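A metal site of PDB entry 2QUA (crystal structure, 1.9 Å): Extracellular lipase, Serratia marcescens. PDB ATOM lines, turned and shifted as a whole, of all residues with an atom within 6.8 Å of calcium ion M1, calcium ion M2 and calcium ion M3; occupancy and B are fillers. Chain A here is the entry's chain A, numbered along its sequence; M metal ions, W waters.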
ATOM      1  N   GLY A 492     -24.092  22.581 -18.152  1.00  0.00           N
ATOM      2  CA  GLY A 492     -24.435  21.177 -18.422  1.00  0.00           C
ATOM      3  C   GLY A 492     -24.531  20.370 -17.134  1.00  0.00           C
ATOM      4  O   GLY A 492     -24.469  20.927 -16.034  1.00  0.00           O
ATOM      5  N   GLY A 493     -24.687  19.052 -17.284  1.00  0.00           N
ATOM      6  CA  GLY A 493     -24.762  18.129 -16.156  1.00  0.00           C
ATOM      7  C   GLY A 493     -23.786  16.971 -16.298  1.00  0.00           C
ATOM      8  O   GLY A 493     -22.754  17.100 -16.954  1.00  0.00           O
ATOM      9  N   ASP A 494     -24.137  15.828 -15.703  1.00  0.00           N
ATOM     10  CA  ASP A 494     -23.307  14.625 -15.717  1.00  0.00           C
ATOM     11  C   ASP A 494     -23.078  14.053 -17.118  1.00  0.00           C
ATOM     12  O   ASP A 494     -22.127  13.309 -17.353  1.00  0.00           O
ATOM     13  CB  ASP A 494     -23.928  13.542 -14.844  1.00  0.00           C
ATOM     14  CG  ASP A 494     -23.813  13.841 -13.355  1.00  0.00           C
ATOM     15  OD1 ASP A 494     -22.923  14.636 -12.984  1.00  0.00           O
ATOM     16  OD2 ASP A 494     -24.599  13.274 -12.563  1.00  0.00           O
ATOM     17  N   GLY A 495     -23.981  14.402 -18.030  1.00  0.00           N
ATOM     18  CA  GLY A 495     -23.943  13.843 -19.387  1.00  0.00           C
ATOM     19  C   GLY A 495     -22.911  14.495 -20.285  1.00  0.00           C
ATOM     20  O   GLY A 495     -22.266  15.478 -19.919  1.00  0.00           O
ATOM     21  N   ASP A 496     -22.759  13.932 -21.471  1.00  0.00           N
ATOM     22  CA  ASP A 496     -21.915  14.474 -22.506  1.00  0.00           C
ATOM     23  C   ASP A 496     -22.749  15.550 -23.188  1.00  0.00           C
ATOM     24  O   ASP A 496     -23.506  15.269 -24.117  1.00  0.00           O
ATOM     25  CB  ASP A 496     -21.510  13.366 -23.489  1.00  0.00           C
ATOM     26  CG  ASP A 496     -20.802  12.197 -22.795  1.00  0.00           C
ATOM     27  OD1 ASP A 496     -20.281  12.383 -21.671  1.00  0.00           O
ATOM     28  OD2 ASP A 496     -20.762  11.098 -23.368  1.00  0.00           O
ATOM     29  N   ASP A 497     -22.601  16.783 -22.713  1.00  0.00           N
ATOM     30  CA  ASP A 497     -23.446  17.890 -23.148  1.00  0.00           C
ATOM     31  C   ASP A 497     -22.870  18.654 -24.340  1.00  0.00           C
ATOM     32  O   ASP A 497     -21.652  18.825 -24.461  1.00  0.00           O
ATOM     33  CB  ASP A 497     -23.636  18.864 -21.986  1.00  0.00           C
ATOM     34  CG  ASP A 497     -24.154  18.179 -20.737  1.00  0.00           C
ATOM     35  OD1 ASP A 497     -25.231  17.559 -20.820  1.00  0.00           O
ATOM     36  OD2 ASP A 497     -23.485  18.262 -19.688  1.00  0.00           O
ATOM     37  N   LEU A 499     -22.950  22.375 -25.502  1.00  0.00           N
ATOM     38  CA  LEU A 499     -23.300  23.713 -25.041  1.00  0.00           C
ATOM     39  C   LEU A 499     -22.920  24.790 -26.047  1.00  0.00           C
ATOM     40  O   LEU A 499     -21.731  25.046 -26.270  1.00  0.00           O
ATOM     41  CB  LEU A 499     -22.612  24.010 -23.701  1.00  0.00           C
ATOM     42  CG  LEU A 499     -22.933  23.044 -22.566  1.00  0.00           C
ATOM     43  CD1 LEU A 499     -22.212  23.439 -21.286  1.00  0.00           C
ATOM     44  CD2 LEU A 499     -24.431  23.007 -22.367  1.00  0.00           C
ATOM     45  N   PHE A 509     -20.137  25.881 -18.603  1.00  0.00           N
ATOM     46  CA  PHE A 509     -19.737  24.833 -17.672  1.00  0.00           C
ATOM     47  C   PHE A 509     -20.206  23.473 -18.190  1.00  0.00           C
ATOM     48  O   PHE A 509     -21.405  23.187 -18.183  1.00  0.00           O
ATOM     49  CB  PHE A 509     -20.369  25.080 -16.304  1.00  0.00           C
ATOM     50  CG  PHE A 509     -19.973  26.390 -15.656  1.00  0.00           C
ATOM     51  CD1 PHE A 509     -18.657  26.626 -15.264  1.00  0.00           C
ATOM     52  CD2 PHE A 509     -20.919  27.382 -15.438  1.00  0.00           C
ATOM     53  CE1 PHE A 509     -18.305  27.839 -14.652  1.00  0.00           C
ATOM     54  CE2 PHE A 509     -20.575  28.584 -14.829  1.00  0.00           C
ATOM     55  CZ  PHE A 509     -19.269  28.802 -14.446  1.00  0.00           C
ATOM     56  N   GLY A 510     -19.274  22.643 -18.650  1.00  0.00           N
ATOM     57  CA  GLY A 510     -19.619  21.316 -19.124  1.00  0.00           C
ATOM     58  C   GLY A 510     -19.953  20.384 -17.966  1.00  0.00           C
ATOM     59  O   GLY A 510     -20.807  19.523 -18.103  1.00  0.00           O
ATOM     60  N   ASN A 511     -19.269  20.578 -16.832  1.00  0.00           N
ATOM     61  CA  ASN A 511     -19.382  19.673 -15.676  1.00  0.00           C
ATOM     62  C   ASN A 511     -18.899  18.276 -16.059  1.00  0.00           C
ATOM     63  O   ASN A 511     -18.067  18.148 -16.956  1.00  0.00           O
ATOM     64  CB  ASN A 511     -20.821  19.679 -15.091  1.00  0.00           C
ATOM     65  CG  ASN A 511     -21.124  20.965 -14.286  1.00  0.00           C
ATOM     66  OD1 ASN A 511     -20.270  21.467 -13.569  1.00  0.00           O
ATOM     67  ND2 ASN A 511     -22.341  21.489 -14.411  1.00  0.00           N
ATOM     68  N   ALA A 512     -19.384  17.239 -15.409  1.00  0.00           N
ATOM     69  CA  ALA A 512     -18.881  15.887 -15.692  1.00  0.00           C
ATOM     70  C   ALA A 512     -19.221  15.434 -17.104  1.00  0.00           C
ATOM     71  O   ALA A 512     -20.084  16.009 -17.773  1.00  0.00           O
ATOM     72  CB  ALA A 512     -19.407  14.889 -14.677  1.00  0.00           C
ATOM     73  N   GLY A 513     -18.541  14.389 -17.567  1.00  0.00           N
ATOM     74  CA  GLY A 513     -18.792  13.870 -18.904  1.00  0.00           C
ATOM     75  C   GLY A 513     -17.984  14.601 -19.962  1.00  0.00           C
ATOM     76  O   GLY A 513     -17.273  15.582 -19.677  1.00  0.00           O
ATOM     77  N   ASN A 514     -18.102  14.121 -21.182  1.00  0.00           N
ATOM     78  CA  ASN A 514     -17.346  14.656 -22.312  1.00  0.00           C
ATOM     79  C   ASN A 514     -18.207  15.661 -23.080  1.00  0.00           C
ATOM     80  O   ASN A 514     -19.069  15.289 -23.875  1.00  0.00           O
ATOM     81  CB  ASN A 514     -16.831  13.503 -23.186  1.00  0.00           C
ATOM     82  CG  ASN A 514     -15.905  12.564 -22.408  1.00  0.00           C
ATOM     83  OD1 ASN A 514     -15.542  12.825 -21.254  1.00  0.00           O
ATOM     84  ND2 ASN A 514     -15.511  11.474 -23.049  1.00  0.00           N
ATOM     85  N   ASP A 515     -17.951  16.932 -22.816  1.00  0.00           N
ATOM     86  CA  ASP A 515     -18.790  18.017 -23.304  1.00  0.00           C
ATOM     87  C   ASP A 515     -18.195  18.773 -24.487  1.00  0.00           C
ATOM     88  O   ASP A 515     -16.963  18.844 -24.645  1.00  0.00           O
ATOM     89  CB  ASP A 515     -18.989  19.011 -22.149  1.00  0.00           C
ATOM     90  CG  ASP A 515     -19.556  18.347 -20.892  1.00  0.00           C
ATOM     91  OD1 ASP A 515     -20.667  17.813 -20.966  1.00  0.00           O
ATOM     92  OD2 ASP A 515     -18.878  18.374 -19.838  1.00  0.00           O
ATOM     93  N   LEU A 517     -18.215  22.545 -25.906  1.00  0.00           N
ATOM     94  CA  LEU A 517     -18.501  23.946 -25.588  1.00  0.00           C
ATOM     95  C   LEU A 517     -18.156  24.837 -26.775  1.00  0.00           C
ATOM     96  O   LEU A 517     -16.994  24.878 -27.208  1.00  0.00           O
ATOM     97  CB  LEU A 517     -17.705  24.402 -24.355  1.00  0.00           C
ATOM     98  CG  LEU A 517     -18.127  23.960 -22.951  1.00  0.00           C
ATOM     99  CD1 LEU A 517     -18.360  22.465 -22.866  1.00  0.00           C
ATOM    100  CD2 LEU A 517     -17.079  24.389 -21.909  1.00  0.00           C
ATOM    101  N   VAL A 528     -15.208  26.294 -19.316  1.00  0.00           N
ATOM    102  CA  VAL A 528     -14.816  25.396 -18.250  1.00  0.00           C
ATOM    103  C   VAL A 528     -15.342  24.005 -18.586  1.00  0.00           C
ATOM    104  O   VAL A 528     -16.520  23.702 -18.322  1.00  0.00           O
ATOM    105  CB  VAL A 528     -15.427  25.835 -16.927  1.00  0.00           C
ATOM    106  CG1 VAL A 528     -14.800  25.036 -15.780  1.00  0.00           C
ATOM    107  CG2 VAL A 528     -15.267  27.341 -16.738  1.00  0.00           C
ATOM    108  N   GLY A 529     -14.512  23.154 -19.187  1.00  0.00           N
ATOM    109  CA  GLY A 529     -15.020  21.835 -19.610  1.00  0.00           C
ATOM    110  C   GLY A 529     -15.365  20.945 -18.423  1.00  0.00           C
ATOM    111  O   GLY A 529     -16.246  20.076 -18.502  1.00  0.00           O
ATOM    112  N   GLY A 530     -14.672  21.193 -17.309  1.00  0.00           N
ATOM    113  CA  GLY A 530     -14.861  20.451 -16.078  1.00  0.00           C
ATOM    114  C   GLY A 530     -14.173  19.103 -16.205  1.00  0.00           C
ATOM    115  O   GLY A 530     -13.322  18.923 -17.071  1.00  0.00           O
ATOM    116  N   SER A 531     -14.543  18.168 -15.356  1.00  0.00           N
ATOM    117  CA  SER A 531     -14.002  16.824 -15.477  1.00  0.00           C
ATOM    118  C   SER A 531     -14.503  16.202 -16.782  1.00  0.00           C
ATOM    119  O   SER A 531     -15.407  16.742 -17.438  1.00  0.00           O
ATOM    120  CB  SER A 531     -14.381  15.960 -14.273  1.00  0.00           C
ATOM    121  OG  SER A 531     -15.745  15.604 -14.326  1.00  0.00           O
ATOM    122  N   GLY A 532     -13.909  15.078 -17.160  1.00  0.00           N
ATOM    123  CA  GLY A 532     -14.185  14.448 -18.454  1.00  0.00           C
ATOM    124  C   GLY A 532     -13.359  15.088 -19.560  1.00  0.00           C
ATOM    125  O   GLY A 532     -12.657  16.101 -19.376  1.00  0.00           O
ATOM    126  N   ASP A 533     -13.444  14.493 -20.737  1.00  0.00           N
ATOM    127  CA  ASP A 533     -12.644  14.915 -21.876  1.00  0.00           C
ATOM    128  C   ASP A 533     -13.480  15.769 -22.792  1.00  0.00           C
ATOM    129  O   ASP A 533     -14.372  15.264 -23.470  1.00  0.00           O
ATOM    130  CB  ASP A 533     -12.108  13.705 -22.617  1.00  0.00           C
ATOM    131  CG  ASP A 533     -11.287  12.801 -21.718  1.00  0.00           C
ATOM    132  OD1 ASP A 533     -10.790  13.275 -20.674  1.00  0.00           O
ATOM    133  OD2 ASP A 533     -11.122  11.606 -22.057  1.00  0.00           O
ATOM    134  N   ASP A 534     -13.172  17.066 -22.800  1.00  0.00           N
ATOM    135  CA  ASP A 534     -14.047  18.070 -23.423  1.00  0.00           C
ATOM    136  C   ASP A 534     -13.454  18.720 -24.682  1.00  0.00           C
ATOM    137  O   ASP A 534     -12.250  18.810 -24.862  1.00  0.00           O
ATOM    138  CB  ASP A 534     -14.392  19.162 -22.394  1.00  0.00           C
ATOM    139  CG  ASP A 534     -14.955  18.590 -21.090  1.00  0.00           C
ATOM    140  OD1 ASP A 534     -16.081  18.052 -21.097  1.00  0.00           O
ATOM    141  OD2 ASP A 534     -14.274  18.655 -20.051  1.00  0.00           O
ATOM    142  N   LEU A 536     -13.376  22.227 -26.748  1.00  0.00           N
ATOM    143  CA  LEU A 536     -13.550  23.663 -26.511  1.00  0.00           C
ATOM    144  C   LEU A 536     -13.346  24.461 -27.796  1.00  0.00           C
ATOM    145  O   LEU A 536     -12.220  24.579 -28.303  1.00  0.00           O
ATOM    146  CB  LEU A 536     -12.580  24.172 -25.434  1.00  0.00           C
ATOM    147  CG  LEU A 536     -12.392  23.225 -24.247  1.00  0.00           C
ATOM    148  CD1 LEU A 536     -11.150  23.654 -23.408  1.00  0.00           C
ATOM    149  CD2 LEU A 536     -13.667  23.118 -23.381  1.00  0.00           C
ATOM    150  N   PHE A 547      -9.032  25.577 -16.345  1.00  0.00           N
ATOM    151  CA  PHE A 547      -8.786  24.176 -15.998  1.00  0.00           C
ATOM    152  C   PHE A 547      -8.342  24.091 -14.555  1.00  0.00           C
ATOM    153  O   PHE A 547      -7.446  24.844 -14.148  1.00  0.00           O
ATOM    154  CB  PHE A 547      -7.661  23.602 -16.862  1.00  0.00           C
ATOM    155  CG  PHE A 547      -7.840  23.870 -18.326  1.00  0.00           C
ATOM    156  CD1 PHE A 547      -8.506  22.953 -19.117  1.00  0.00           C
ATOM    157  CD2 PHE A 547      -7.362  25.040 -18.900  1.00  0.00           C
ATOM    158  CE1 PHE A 547      -8.694  23.197 -20.490  1.00  0.00           C
ATOM    159  CE2 PHE A 547      -7.546  25.300 -20.277  1.00  0.00           C
ATOM    160  CZ  PHE A 547      -8.207  24.370 -21.068  1.00  0.00           C
ATOM    161  N   ASP A 550      -8.207  17.685 -11.468  1.00  0.00           N
ATOM    162  CA  ASP A 550      -8.127  16.699 -12.529  1.00  0.00           C
ATOM    163  C   ASP A 550      -9.144  17.045 -13.618  1.00  0.00           C
ATOM    164  O   ASP A 550     -10.300  16.625 -13.561  1.00  0.00           O
ATOM    165  CB  ASP A 550      -8.322  15.286 -11.978  1.00  0.00           C
ATOM    166  CG  ASP A 550      -7.250  14.921 -10.932  1.00  0.00           C
ATOM    167  OD1 ASP A 550      -6.041  15.039 -11.258  1.00  0.00           O
ATOM    168  OD2 ASP A 550      -7.616  14.528  -9.798  1.00  0.00           O
ATOM    169  N   PHE A 551      -8.708  17.812 -14.615  1.00  0.00           N
ATOM    170  CA  PHE A 551      -9.624  18.319 -15.623  1.00  0.00           C
ATOM    171  C   PHE A 551      -9.739  17.422 -16.873  1.00  0.00           C
ATOM    172  O   PHE A 551     -10.319  17.838 -17.857  1.00  0.00           O
ATOM    173  CB  PHE A 551      -9.275  19.778 -16.004  1.00  0.00           C
ATOM    174  CG  PHE A 551      -7.903  19.937 -16.595  1.00  0.00           C
ATOM    175  CD1 PHE A 551      -6.802  20.186 -15.762  1.00  0.00           C
ATOM    176  CD2 PHE A 551      -7.691  19.843 -17.977  1.00  0.00           C
ATOM    177  CE1 PHE A 551      -5.524  20.330 -16.297  1.00  0.00           C
ATOM    178  CE2 PHE A 551      -6.414  19.979 -18.518  1.00  0.00           C
ATOM    179  CZ  PHE A 551      -5.322  20.225 -17.682  1.00  0.00           C
ATOM    180  N   GLY A 552      -9.205  16.206 -16.819  1.00  0.00           N
ATOM    181  CA  GLY A 552      -9.300  15.267 -17.955  1.00  0.00           C
ATOM    182  C   GLY A 552      -8.490  15.705 -19.161  1.00  0.00           C
ATOM    183  O   GLY A 552      -7.566  16.507 -19.036  1.00  0.00           O
ATOM    184  N   ARG A 553      -8.835  15.197 -20.346  1.00  0.00           N
ATOM    185  CA  ARG A 553      -8.033  15.500 -21.513  1.00  0.00           C
ATOM    186  C   ARG A 553      -8.824  16.277 -22.560  1.00  0.00           C
ATOM    187  O   ARG A 553      -9.638  15.692 -23.272  1.00  0.00           O
ATOM    188  CB  ARG A 553      -7.499  14.195 -22.124  1.00  0.00           C
ATOM    189  CG  ARG A 553      -6.713  13.327 -21.124  1.00  0.00           C
ATOM    190  CD  ARG A 553      -5.973  12.169 -21.833  1.00  0.00           C
ATOM    191  NE  ARG A 553      -5.485  11.173 -20.876  1.00  0.00           N
ATOM    192  CZ  ARG A 553      -4.390  11.307 -20.109  1.00  0.00           C
ATOM    193  NH1 ARG A 553      -3.648  12.417 -20.172  1.00  0.00           N
ATOM    194  NH2 ARG A 553      -4.035  10.332 -19.279  1.00  0.00           N
ATOM    195  N   ASP A 554      -8.567  17.571 -22.655  1.00  0.00           N
ATOM    196  CA  ASP A 554      -9.366  18.461 -23.491  1.00  0.00           C
ATOM    197  C   ASP A 554      -8.701  18.738 -24.853  1.00  0.00           C
ATOM    198  O   ASP A 554      -7.483  18.633 -24.986  1.00  0.00           O
ATOM    199  CB  ASP A 554      -9.548  19.807 -22.783  1.00  0.00           C
ATOM    200  CG  ASP A 554     -10.595  19.788 -21.630  1.00  0.00           C
ATOM    201  OD1 ASP A 554     -10.974  18.725 -21.065  1.00  0.00           O
ATOM    202  OD2 ASP A 554     -11.066  20.899 -21.292  1.00  0.00           O
ATOM    203  N   GLN A 596      -4.705  16.994 -19.596  1.00  0.00           N
ATOM    204  CA  GLN A 596      -3.913  17.662 -20.607  1.00  0.00           C
ATOM    205  C   GLN A 596      -4.813  18.482 -21.462  1.00  0.00           C
ATOM    206  O   GLN A 596      -6.029  18.265 -21.473  1.00  0.00           O
ATOM    207  CB  GLN A 596      -3.164  16.638 -21.480  1.00  0.00           C
ATOM    208  CG  GLN A 596      -4.039  15.960 -22.516  1.00  0.00           C
ATOM    209  CD  GLN A 596      -3.296  14.920 -23.337  1.00  0.00           C
ATOM    210  OE1 GLN A 596      -2.532  14.109 -22.799  1.00  0.00           O
ATOM    211  NE2 GLN A 596      -3.509  14.927 -24.655  1.00  0.00           N
HETATM  212 CA    CA M   1     -12.196  18.392 -19.059  1.00  0.00          CA
HETATM  213 CA    CA M   2     -16.855  17.817 -18.895  1.00  0.00          CA
HETATM  214 CA    CA M   3     -21.499  17.438 -18.859  1.00  0.00          CA
HETATM  215  O   HOH W   1     -11.721  20.677 -18.894  1.00  0.00           O
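Calcium ion M2 is bound by the side-chain carboxylate of Asp 515 (2.3 Å), the backbone carbonyl oxygen of Asn 511 (2.3 Å), the backbone carbonyl oxygen of Ser 531 (2.3 Å), the side-chain carboxylate of Asp 534 (2.3 Å), the backbone carbonyl oxygen of Gly 529 (2.4 Å) and the backbone carbonyl oxygen of Gly 513 (2.4 Å).
Calcium ion M2 has six donor atoms within binding distance.
Slightly farther from calcium ion M2 lies OD2 of Asp 534 (2.9 Å).
O of Phe 551 binds calcium ion M1 (2.3 Å).
OD2 of Asp 534 binds calcium ion M1, at 2.3 Å.
Calcium ion M1 is bound by water W1 (2.3 Å).
O of Gly 530 is bound to calcium ion M1 (2.3 Å).
The backbone carbonyl oxygen (O) of Gly 532 binds calcium ion M1 (2.4 Å).
The side-chain carboxylate (OD1) of Asp 554 is bound to calcium ion M1, 2.4 Å away.
Calcium ion M1 has six donor atoms within binding distance.
Calcium ion M3 is bound by the backbone carbonyl oxygen of Ala 512 (2.3 Å), the side-chain carboxylate of Asp 515 (2.3 Å), the side-chain carboxylate of Asp 497 (2.3 Å), the backbone carbonyl oxygen of Gly 493 (2.3 Å), the backbone carbonyl oxygen of Gly 510 (2.3 Å) and the backbone carbonyl oxygen of Gly 495 (2.4 Å).
Calcium ion M3 has six donor atoms within binding distance.
Slightly farther from calcium ion M3 lies the side-chain carboxylate (OD2) of Asp 515 (3.0 Å).
Of the 30 residues printed, 7 come within 4 Å of calcium ion M2.
O of Gly 492 is in hydrogen-bond range of ND2 of Asn 511.
N of Gly 510 lies within hydrogen-bond range of O of Val 528, 3.0 Å away.
The backbone NH (N) of Asp 554 is in hydrogen-bond range of the backbone carbonyl oxygen (O) of Gln 596 (2.9 Å).
Of the 30 residues printed, 7 come within 4 Å of calcium ion M3.
Within 4 Å of calcium ion M1: Gly 530, Ser 531, Gly 532, Asp 534, Phe 551 and Asp 554.
Water W1 lies within hydrogen-bond range of the side-chain carboxylate of Asp 554 (2.5 Å) and the backbone NH of Gly 530 (3.4 Å).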
